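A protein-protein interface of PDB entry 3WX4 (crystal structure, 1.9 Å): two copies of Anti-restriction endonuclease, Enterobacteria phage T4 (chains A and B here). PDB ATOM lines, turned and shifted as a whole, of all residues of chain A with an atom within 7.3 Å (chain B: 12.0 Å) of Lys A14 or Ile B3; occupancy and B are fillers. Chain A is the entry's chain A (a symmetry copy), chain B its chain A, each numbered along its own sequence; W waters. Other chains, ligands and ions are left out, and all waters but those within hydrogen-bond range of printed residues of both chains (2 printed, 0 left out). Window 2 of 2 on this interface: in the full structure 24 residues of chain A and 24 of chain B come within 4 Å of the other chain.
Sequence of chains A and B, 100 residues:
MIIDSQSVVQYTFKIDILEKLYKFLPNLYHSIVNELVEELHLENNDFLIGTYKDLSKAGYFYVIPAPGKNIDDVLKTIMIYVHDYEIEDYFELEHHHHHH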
ATOM      1  N   TYR A  11      -4.047   4.078 -11.631  1.00  0.00           N
ATOM      2  CA  TYR A  11      -3.335   3.874 -10.380  1.00  0.00           C
ATOM      3  C   TYR A  11      -4.063   4.539  -9.215  1.00  0.00           C
ATOM      4  O   TYR A  11      -4.778   5.512  -9.435  1.00  0.00           O
ATOM      5  CB  TYR A  11      -1.946   4.512 -10.455  1.00  0.00           C
ATOM      6  CG  TYR A  11      -1.065   3.890 -11.496  1.00  0.00           C
ATOM      7  CD1 TYR A  11      -0.313   2.768 -11.195  1.00  0.00           C
ATOM      8  CD2 TYR A  11      -1.057   4.360 -12.812  1.00  0.00           C
ATOM      9  CE1 TYR A  11       0.431   2.102 -12.190  1.00  0.00           C
ATOM     10  CE2 TYR A  11      -0.314   3.698 -13.807  1.00  0.00           C
ATOM     11  CZ  TYR A  11       0.418   2.563 -13.470  1.00  0.00           C
ATOM     12  OH  TYR A  11       1.097   1.822 -14.431  1.00  0.00           O
ATOM     13  N   THR A  12      -3.865   4.004  -8.005  1.00  0.00           N
ATOM     14  CA  THR A  12      -4.401   4.620  -6.796  1.00  0.00           C
ATOM     15  C   THR A  12      -3.152   5.130  -6.110  1.00  0.00           C
ATOM     16  O   THR A  12      -2.265   4.354  -5.713  1.00  0.00           O
ATOM     17  CB  THR A  12      -5.111   3.624  -5.903  1.00  0.00           C
ATOM     18  OG1 THR A  12      -6.286   3.188  -6.557  1.00  0.00           O
ATOM     19  CG2 THR A  12      -5.494   4.272  -4.592  1.00  0.00           C
ATOM     20  N   PHE A  13      -3.046   6.441  -6.024  1.00  0.00           N
ATOM     21  CA  PHE A  13      -1.897   7.072  -5.417  1.00  0.00           C
ATOM     22  C   PHE A  13      -2.339   7.618  -4.059  1.00  0.00           C
ATOM     23  O   PHE A  13      -3.273   8.414  -4.008  1.00  0.00           O
ATOM     24  CB  PHE A  13      -1.435   8.225  -6.323  1.00  0.00           C
ATOM     25  CG  PHE A  13      -0.173   8.876  -5.871  1.00  0.00           C
ATOM     26  CD1 PHE A  13      -0.091  10.263  -5.764  1.00  0.00           C
ATOM     27  CD2 PHE A  13       0.957   8.106  -5.563  1.00  0.00           C
ATOM     28  CE1 PHE A  13       1.080  10.894  -5.360  1.00  0.00           C
ATOM     29  CE2 PHE A  13       2.153   8.707  -5.158  1.00  0.00           C
ATOM     30  CZ  PHE A  13       2.231  10.119  -5.051  1.00  0.00           C
ATOM     31  N   LYS A  14      -1.698   7.185  -2.974  1.00  0.00           N
ATOM     32  CA  LYS A  14      -2.043   7.670  -1.641  1.00  0.00           C
ATOM     33  C   LYS A  14      -1.142   8.804  -1.295  1.00  0.00           C
ATOM     34  O   LYS A  14       0.079   8.691  -1.414  1.00  0.00           O
ATOM     35  CB  LYS A  14      -1.862   6.566  -0.610  1.00  0.00           C
ATOM     36  CG  LYS A  14      -2.165   6.946   0.848  1.00  0.00           C
ATOM     37  CD  LYS A  14      -2.205   5.615   1.661  1.00  0.00           C
ATOM     38  CE  LYS A  14      -2.054   5.850   3.125  1.00  0.00           C
ATOM     39  NZ  LYS A  14      -1.795   4.571   3.809  1.00  0.00           N
ATOM     40  N   ILE A  15      -1.715   9.928  -0.884  1.00  0.00           N
ATOM     41  CA  ILE A  15      -0.898  11.042  -0.529  1.00  0.00           C
ATOM     42  C   ILE A  15      -1.075  11.152   0.954  1.00  0.00           C
ATOM     43  O   ILE A  15      -2.075  11.697   1.460  1.00  0.00           O
ATOM     44  CB  ILE A  15      -1.321  12.311  -1.301  1.00  0.00           C
ATOM     45  CG1 ILE A  15      -1.193  12.058  -2.800  1.00  0.00           C
ATOM     46  CG2 ILE A  15      -0.441  13.468  -0.921  1.00  0.00           C
ATOM     47  CD1 ILE A  15      -1.621  13.242  -3.679  1.00  0.00           C
ATOM     48  N   ASP A  16      -0.116  10.578   1.686  1.00  0.00           N
ATOM     49  CA  ASP A  16      -0.187  10.580   3.150  1.00  0.00           C
ATOM     50  C   ASP A  16      -0.525  11.920   3.851  1.00  0.00           C
ATOM     51  O   ASP A  16      -1.420  11.970   4.721  1.00  0.00           O
ATOM     52  CB  ASP A  16       1.137  10.093   3.742  1.00  0.00           C
ATOM     53  CG  ASP A  16       1.491   8.623   3.341  1.00  0.00           C
ATOM     54  OD1 ASP A  16       0.619   7.830   2.856  1.00  0.00           O
ATOM     55  OD2 ASP A  16       2.687   8.274   3.556  1.00  0.00           O
ATOM     56  N   ILE A  17       0.204  12.987   3.524  1.00  0.00           N
ATOM     57  CA  ILE A  17      -0.042  14.234   4.215  1.00  0.00           C
ATOM     58  C   ILE A  17      -1.468  14.766   3.973  1.00  0.00           C
ATOM     59  O   ILE A  17      -2.026  15.448   4.849  1.00  0.00           O
ATOM     60  CB  ILE A  17       1.010  15.310   3.874  1.00  0.00           C
ATOM     61  CG1 ILE A  17       1.033  16.335   4.984  1.00  0.00           C
ATOM     62  CG2 ILE A  17       0.716  15.996   2.517  1.00  0.00           C
ATOM     63  CD1 ILE A  17       2.292  17.256   4.982  1.00  0.00           C
ATOM     64  N   LEU A  18      -2.057  14.436   2.823  1.00  0.00           N
ATOM     65  CA  LEU A  18      -3.439  14.923   2.545  1.00  0.00           C
ATOM     66  C   LEU A  18      -4.418  14.067   3.293  1.00  0.00           C
ATOM     67  O   LEU A  18      -5.443  14.585   3.789  1.00  0.00           O
ATOM     68  CB  LEU A  18      -3.794  14.894   1.047  1.00  0.00           C
ATOM     69  CG  LEU A  18      -3.229  16.122   0.301  1.00  0.00           C
ATOM     70  CD1 LEU A  18      -3.373  15.869  -1.234  1.00  0.00           C
ATOM     71  CD2 LEU A  18      -3.943  17.451   0.747  1.00  0.00           C
ATOM     72  N   GLU A  19      -4.138  12.751   3.364  1.00  0.00           N
ATOM     73  CA  GLU A  19      -5.028  11.882   4.133  1.00  0.00           C
ATOM     74  C   GLU A  19      -5.024  12.357   5.600  1.00  0.00           C
ATOM     75  O   GLU A  19      -6.076  12.422   6.245  1.00  0.00           O
ATOM     76  CB  GLU A  19      -4.566  10.425   4.103  1.00  0.00           C
ATOM     77  CG  GLU A  19      -5.374   9.522   5.029  1.00  0.00           C
ATOM     78  CD  GLU A  19      -4.920   8.071   4.977  1.00  0.00           C
ATOM     79  OE1 GLU A  19      -3.668   7.876   5.082  1.00  0.00           O
ATOM     80  OE2 GLU A  19      -5.788   7.175   4.837  1.00  0.00           O
ATOM     81  N   LYS A  57     -11.338   6.664   1.506  1.00  0.00           N
ATOM     82  CA  LYS A  57     -10.220   6.840   0.590  1.00  0.00           C
ATOM     83  C   LYS A  57      -9.810   8.284   0.473  1.00  0.00           C
ATOM     84  O   LYS A  57      -9.098   8.647  -0.500  1.00  0.00           O
ATOM     85  CB  LYS A  57     -10.585   6.326  -0.775  1.00  0.00           C
ATOM     86  CG  LYS A  57     -10.783   4.811  -0.810  1.00  0.00           C
ATOM     87  CD  LYS A  57     -11.214   4.423  -2.250  1.00  0.00           C
ATOM     88  CE  LYS A  57     -11.417   2.894  -2.412  1.00  0.00           C
ATOM     89  NZ  LYS A  57     -12.180   2.275  -1.266  1.00  0.00           N
ATOM     90  N   ALA A  58     -10.241   9.123   1.430  1.00  0.00           N
ATOM     91  CA  ALA A  58      -9.834  10.529   1.363  1.00  0.00           C
ATOM     92  C   ALA A  58      -8.297  10.538   1.350  1.00  0.00           C
ATOM     93  O   ALA A  58      -7.663   9.710   2.034  1.00  0.00           O
ATOM     94  CB  ALA A  58     -10.364  11.306   2.583  1.00  0.00           C
ATOM     95  N   GLY A  59      -7.689  11.490   0.637  1.00  0.00           N
ATOM     96  CA  GLY A  59      -6.236  11.473   0.543  1.00  0.00           C
ATOM     97  C   GLY A  59      -5.686  10.545  -0.553  1.00  0.00           C
ATOM     98  O   GLY A  59      -4.460  10.560  -0.819  1.00  0.00           O
ATOM     99  N   TYR A  60      -6.534   9.709  -1.161  1.00  0.00           N
ATOM    100  CA  TYR A  60      -6.099   8.833  -2.254  1.00  0.00           C
ATOM    101  C   TYR A  60      -6.638   9.442  -3.540  1.00  0.00           C
ATOM    102  O   TYR A  60      -7.735   9.991  -3.542  1.00  0.00           O
ATOM    103  CB  TYR A  60      -6.716   7.447  -2.233  1.00  0.00           C
ATOM    104  CG  TYR A  60      -6.592   6.601  -0.993  1.00  0.00           C
ATOM    105  CD1 TYR A  60      -5.898   7.028   0.144  1.00  0.00           C
ATOM    106  CD2 TYR A  60      -7.181   5.344  -0.972  1.00  0.00           C
ATOM    107  CE1 TYR A  60      -5.799   6.195   1.276  1.00  0.00           C
ATOM    108  CE2 TYR A  60      -7.085   4.535   0.123  1.00  0.00           C
ATOM    109  CZ  TYR A  60      -6.395   4.969   1.235  1.00  0.00           C
ATOM    110  OH  TYR A  60      -6.311   4.087   2.280  1.00  0.00           O
ATOM    111  N   PHE A  61      -5.905   9.281  -4.642  1.00  0.00           N
ATOM    112  CA  PHE A  61      -6.310   9.831  -5.957  1.00  0.00           C
ATOM    113  C   PHE A  61      -6.220   8.773  -7.021  1.00  0.00           C
ATOM    114  O   PHE A  61      -5.331   7.918  -6.924  1.00  0.00           O
ATOM    115  CB  PHE A  61      -5.380  10.976  -6.330  1.00  0.00           C
ATOM    116  CG  PHE A  61      -5.503  12.123  -5.412  1.00  0.00           C
ATOM    117  CD1 PHE A  61      -6.354  13.174  -5.727  1.00  0.00           C
ATOM    118  CD2 PHE A  61      -4.880  12.093  -4.155  1.00  0.00           C
ATOM    119  CE1 PHE A  61      -6.600  14.186  -4.799  1.00  0.00           C
ATOM    120  CE2 PHE A  61      -5.113  13.091  -3.202  1.00  0.00           C
ATOM    121  CZ  PHE A  61      -5.990  14.151  -3.528  1.00  0.00           C
ATOM    122  N   LEU A  75       3.688  11.223 -10.756  1.00  0.00           N
ATOM    123  CA  LEU A  75       3.688  11.353  -9.308  1.00  0.00           C
ATOM    124  C   LEU A  75       4.572  12.486  -8.847  1.00  0.00           C
ATOM    125  O   LEU A  75       4.252  13.169  -7.907  1.00  0.00           O
ATOM    126  CB  LEU A  75       4.085  10.028  -8.656  1.00  0.00           C
ATOM    127  CG  LEU A  75       3.182   8.864  -9.134  1.00  0.00           C
ATOM    128  CD1 LEU A  75       3.617   7.566  -8.452  1.00  0.00           C
ATOM    129  CD2 LEU A  75       1.706   9.143  -8.846  1.00  0.00           C
ATOM    130  N   MET A  79       3.308  15.631  -6.566  1.00  0.00           N
ATOM    131  CA  MET A  79       3.918  16.026  -5.302  1.00  0.00           C
ATOM    132  C   MET A  79       4.450  17.420  -5.290  1.00  0.00           C
ATOM    133  O   MET A  79       4.398  18.080  -4.259  1.00  0.00           O
ATOM    134  CB  MET A  79       4.986  15.030  -4.862  1.00  0.00           C
ATOM    135  CG  MET A  79       4.417  13.638  -4.653  1.00  0.00           C
ATOM    136  SD  MET A  79       2.981  13.721  -3.408  1.00  0.00           S
ATOM    137  CE  MET A  79       3.815  14.548  -2.059  1.00  0.00           C
ATOM    138  N   MET B   1       2.373   7.123  -1.845  1.00  0.00           N
ATOM    139  CA  MET B   1       2.828   6.202  -2.907  1.00  0.00           C
ATOM    140  C   MET B   1       1.684   5.514  -3.656  1.00  0.00           C
ATOM    141  O   MET B   1       0.506   5.703  -3.354  1.00  0.00           O
ATOM    142  CB  MET B   1       3.743   5.132  -2.310  1.00  0.00           C
ATOM    143  CG  MET B   1       3.089   4.269  -1.251  1.00  0.00           C
ATOM    144  SD  MET B   1       4.105   2.830  -0.676  1.00  0.00           S
ATOM    145  CE  MET B   1       3.011   1.344  -1.102  1.00  0.00           C
ATOM    146  N   ILE B   2       2.047   4.716  -4.652  1.00  0.00           N
ATOM    147  CA  ILE B   2       1.059   3.964  -5.411  1.00  0.00           C
ATOM    148  C   ILE B   2       0.712   2.791  -4.512  1.00  0.00           C
ATOM    149  O   ILE B   2       1.613   2.096  -4.033  1.00  0.00           O
ATOM    150  CB  ILE B   2       1.671   3.435  -6.714  1.00  0.00           C
ATOM    151  CG1 ILE B   2       2.290   4.593  -7.501  1.00  0.00           C
ATOM    152  CG2 ILE B   2       0.648   2.669  -7.492  1.00  0.00           C
ATOM    153  CD1 ILE B   2       1.344   5.283  -8.428  1.00  0.00           C
ATOM    154  N   ILE B   3      -0.573   2.557  -4.268  1.00  0.00           N
ATOM    155  CA  ILE B   3      -0.976   1.472  -3.386  1.00  0.00           C
ATOM    156  C   ILE B   3      -1.909   0.495  -4.030  1.00  0.00           C
ATOM    157  O   ILE B   3      -2.344  -0.463  -3.389  1.00  0.00           O
ATOM    158  CB  ILE B   3      -1.685   1.981  -2.107  1.00  0.00           C
ATOM    159  CG1 ILE B   3      -2.992   2.691  -2.483  1.00  0.00           C
ATOM    160  CG2 ILE B   3      -0.758   2.885  -1.327  1.00  0.00           C
ATOM    161  CD1 ILE B   3      -3.772   3.214  -1.293  1.00  0.00           C
ATOM    162  N   ASP B   4      -2.239   0.736  -5.296  1.00  0.00           N
ATOM    163  CA  ASP B   4      -3.126  -0.165  -6.013  1.00  0.00           C
ATOM    164  C   ASP B   4      -3.220   0.243  -7.480  1.00  0.00           C
ATOM    165  O   ASP B   4      -2.798   1.335  -7.859  1.00  0.00           O
ATOM    166  CB  ASP B   4      -4.508  -0.132  -5.388  1.00  0.00           C
ATOM    167  CG  ASP B   4      -5.312  -1.378  -5.693  1.00  0.00           C
ATOM    168  OD1 ASP B   4      -4.697  -2.416  -6.060  1.00  0.00           O
ATOM    169  OD2 ASP B   4      -6.558  -1.334  -5.548  1.00  0.00           O
ATOM    170  N   SER B   5      -3.773  -0.646  -8.297  1.00  0.00           N
ATOM    171  CA  SER B   5      -3.925  -0.353  -9.711  1.00  0.00           C
ATOM    172  C   SER B   5      -5.032  -1.231 -10.198  1.00  0.00           C
ATOM    173  O   SER B   5      -5.345  -2.249  -9.581  1.00  0.00           O
ATOM    174  CB  SER B   5      -2.637  -0.648 -10.485  1.00  0.00           C
ATOM    175  OG  SER B   5      -2.409  -2.045 -10.581  1.00  0.00           O
ATOM    176  N   GLN B   6      -5.672  -0.808 -11.278  1.00  0.00           N
ATOM    177  CA  GLN B   6      -6.763  -1.565 -11.860  1.00  0.00           C
ATOM    178  C   GLN B   6      -6.812  -1.182 -13.330  1.00  0.00           C
ATOM    179  O   GLN B   6      -6.194  -0.205 -13.748  1.00  0.00           O
ATOM    180  CB  GLN B   6      -8.073  -1.233 -11.162  1.00  0.00           C
ATOM    181  CG  GLN B   6      -8.410   0.235 -11.160  1.00  0.00           C
ATOM    182  CD  GLN B   6      -9.683   0.531 -10.397  1.00  0.00           C
ATOM    183  OE1 GLN B   6     -10.785   0.127 -10.813  1.00  0.00           O
ATOM    184  NE2 GLN B   6      -9.547   1.248  -9.266  1.00  0.00           N
ATOM    185  N   SER B   7      -7.529  -1.973 -14.111  1.00  0.00           N
ATOM    186  CA  SER B   7      -7.629  -1.760 -15.546  1.00  0.00           C
ATOM    187  C   SER B   7      -8.754  -0.810 -15.881  1.00  0.00           C
ATOM    188  O   SER B   7      -9.823  -0.877 -15.285  1.00  0.00           O
ATOM    189  CB  SER B   7      -7.908  -3.087 -16.242  1.00  0.00           C
ATOM    190  OG  SER B   7      -9.283  -3.388 -16.066  1.00  0.00           O
HETATM  191  O   HOH W   1       1.739   6.226   0.763  1.00  0.00           O
HETATM  192  O   HOH W   2      -6.488   1.497  -8.874  1.00  0.00           O
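Water W1 bridges N of Met B1 and OD1 of Asp A16. Water W2 lies within hydrogen-bond range of OG1 of Thr A12 (2.9 Å) and NE2 of Gln B6 (3.1 Å).
Of the 7 printed residues of chain B, 4 touch a printed residue of chain A. Along chain B the printed residues that touch a printed residue of chain A span positions 1 to 4. Of the 16 printed residues of chain A, 6 touch a printed residue of chain B. Among the printed residues, 12 pairs touch across the chains. Among the printed residues, no Asp or Glu carboxylate lies within 4 Å of a Lys or Arg side-chain nitrogen of the other chain.
The backbone carbonyl oxygen (O) of Met B1 is in hydrogen-bond range of the backbone NH (N) of Lys A14. The backbone NH of Ile B3 sits at hydrogen-bond distance from the backbone carbonyl oxygen of Thr A12. The backbone carbonyl oxygen (O) of Asp B4 is in hydrogen-bond range of the backbone NH (N) of Thr A12, at 2.9 Å.
No position is printed for both chains. Of the 12 pairs that touch across the chains among the printed residues, none has its exchanged pair printed and touching as well.
Lys A14 touches just these residues of chain B: Met B1 (2.7 Å) and Ile B3 (3.9 Å). No residue of chain B comes within 4 Å of Ile A15. No residue of chain B comes within 4 Å of Gly A59. Printed residues of chain B within 4 Å of Leu A75: Ile B2. Of the printed residues of chain A, Met B1 touches Thr A12 (3.9 Å), Phe A13 (3.3 Å) and Lys A14 (2.7 Å). Of the printed residues of chain A, Asp B4 touches Tyr A11 and Thr A12. The nearest residue of chain B that does not touch Lys A14 is Ile B2 (4.8 Å). The nearest residue of chain A that does not touch Ile B3 is Phe A13 (4.8 Å).
Among the printed residues, merely in contact across the chains: Tyr A11 with Ile B2, Tyr A11 with Asp B4, Thr A12 with Met B1, Thr A12 with Ile B2, Phe A13 with Met B1, Phe A13 with Ile B2, Lys A14 with Ile B3, Tyr A60 with Ile B3 and Leu A75 with Ile B2.
O of Phe A13 sits at hydrogen-bond distance from N of Phe A61, 2.8 Å away.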
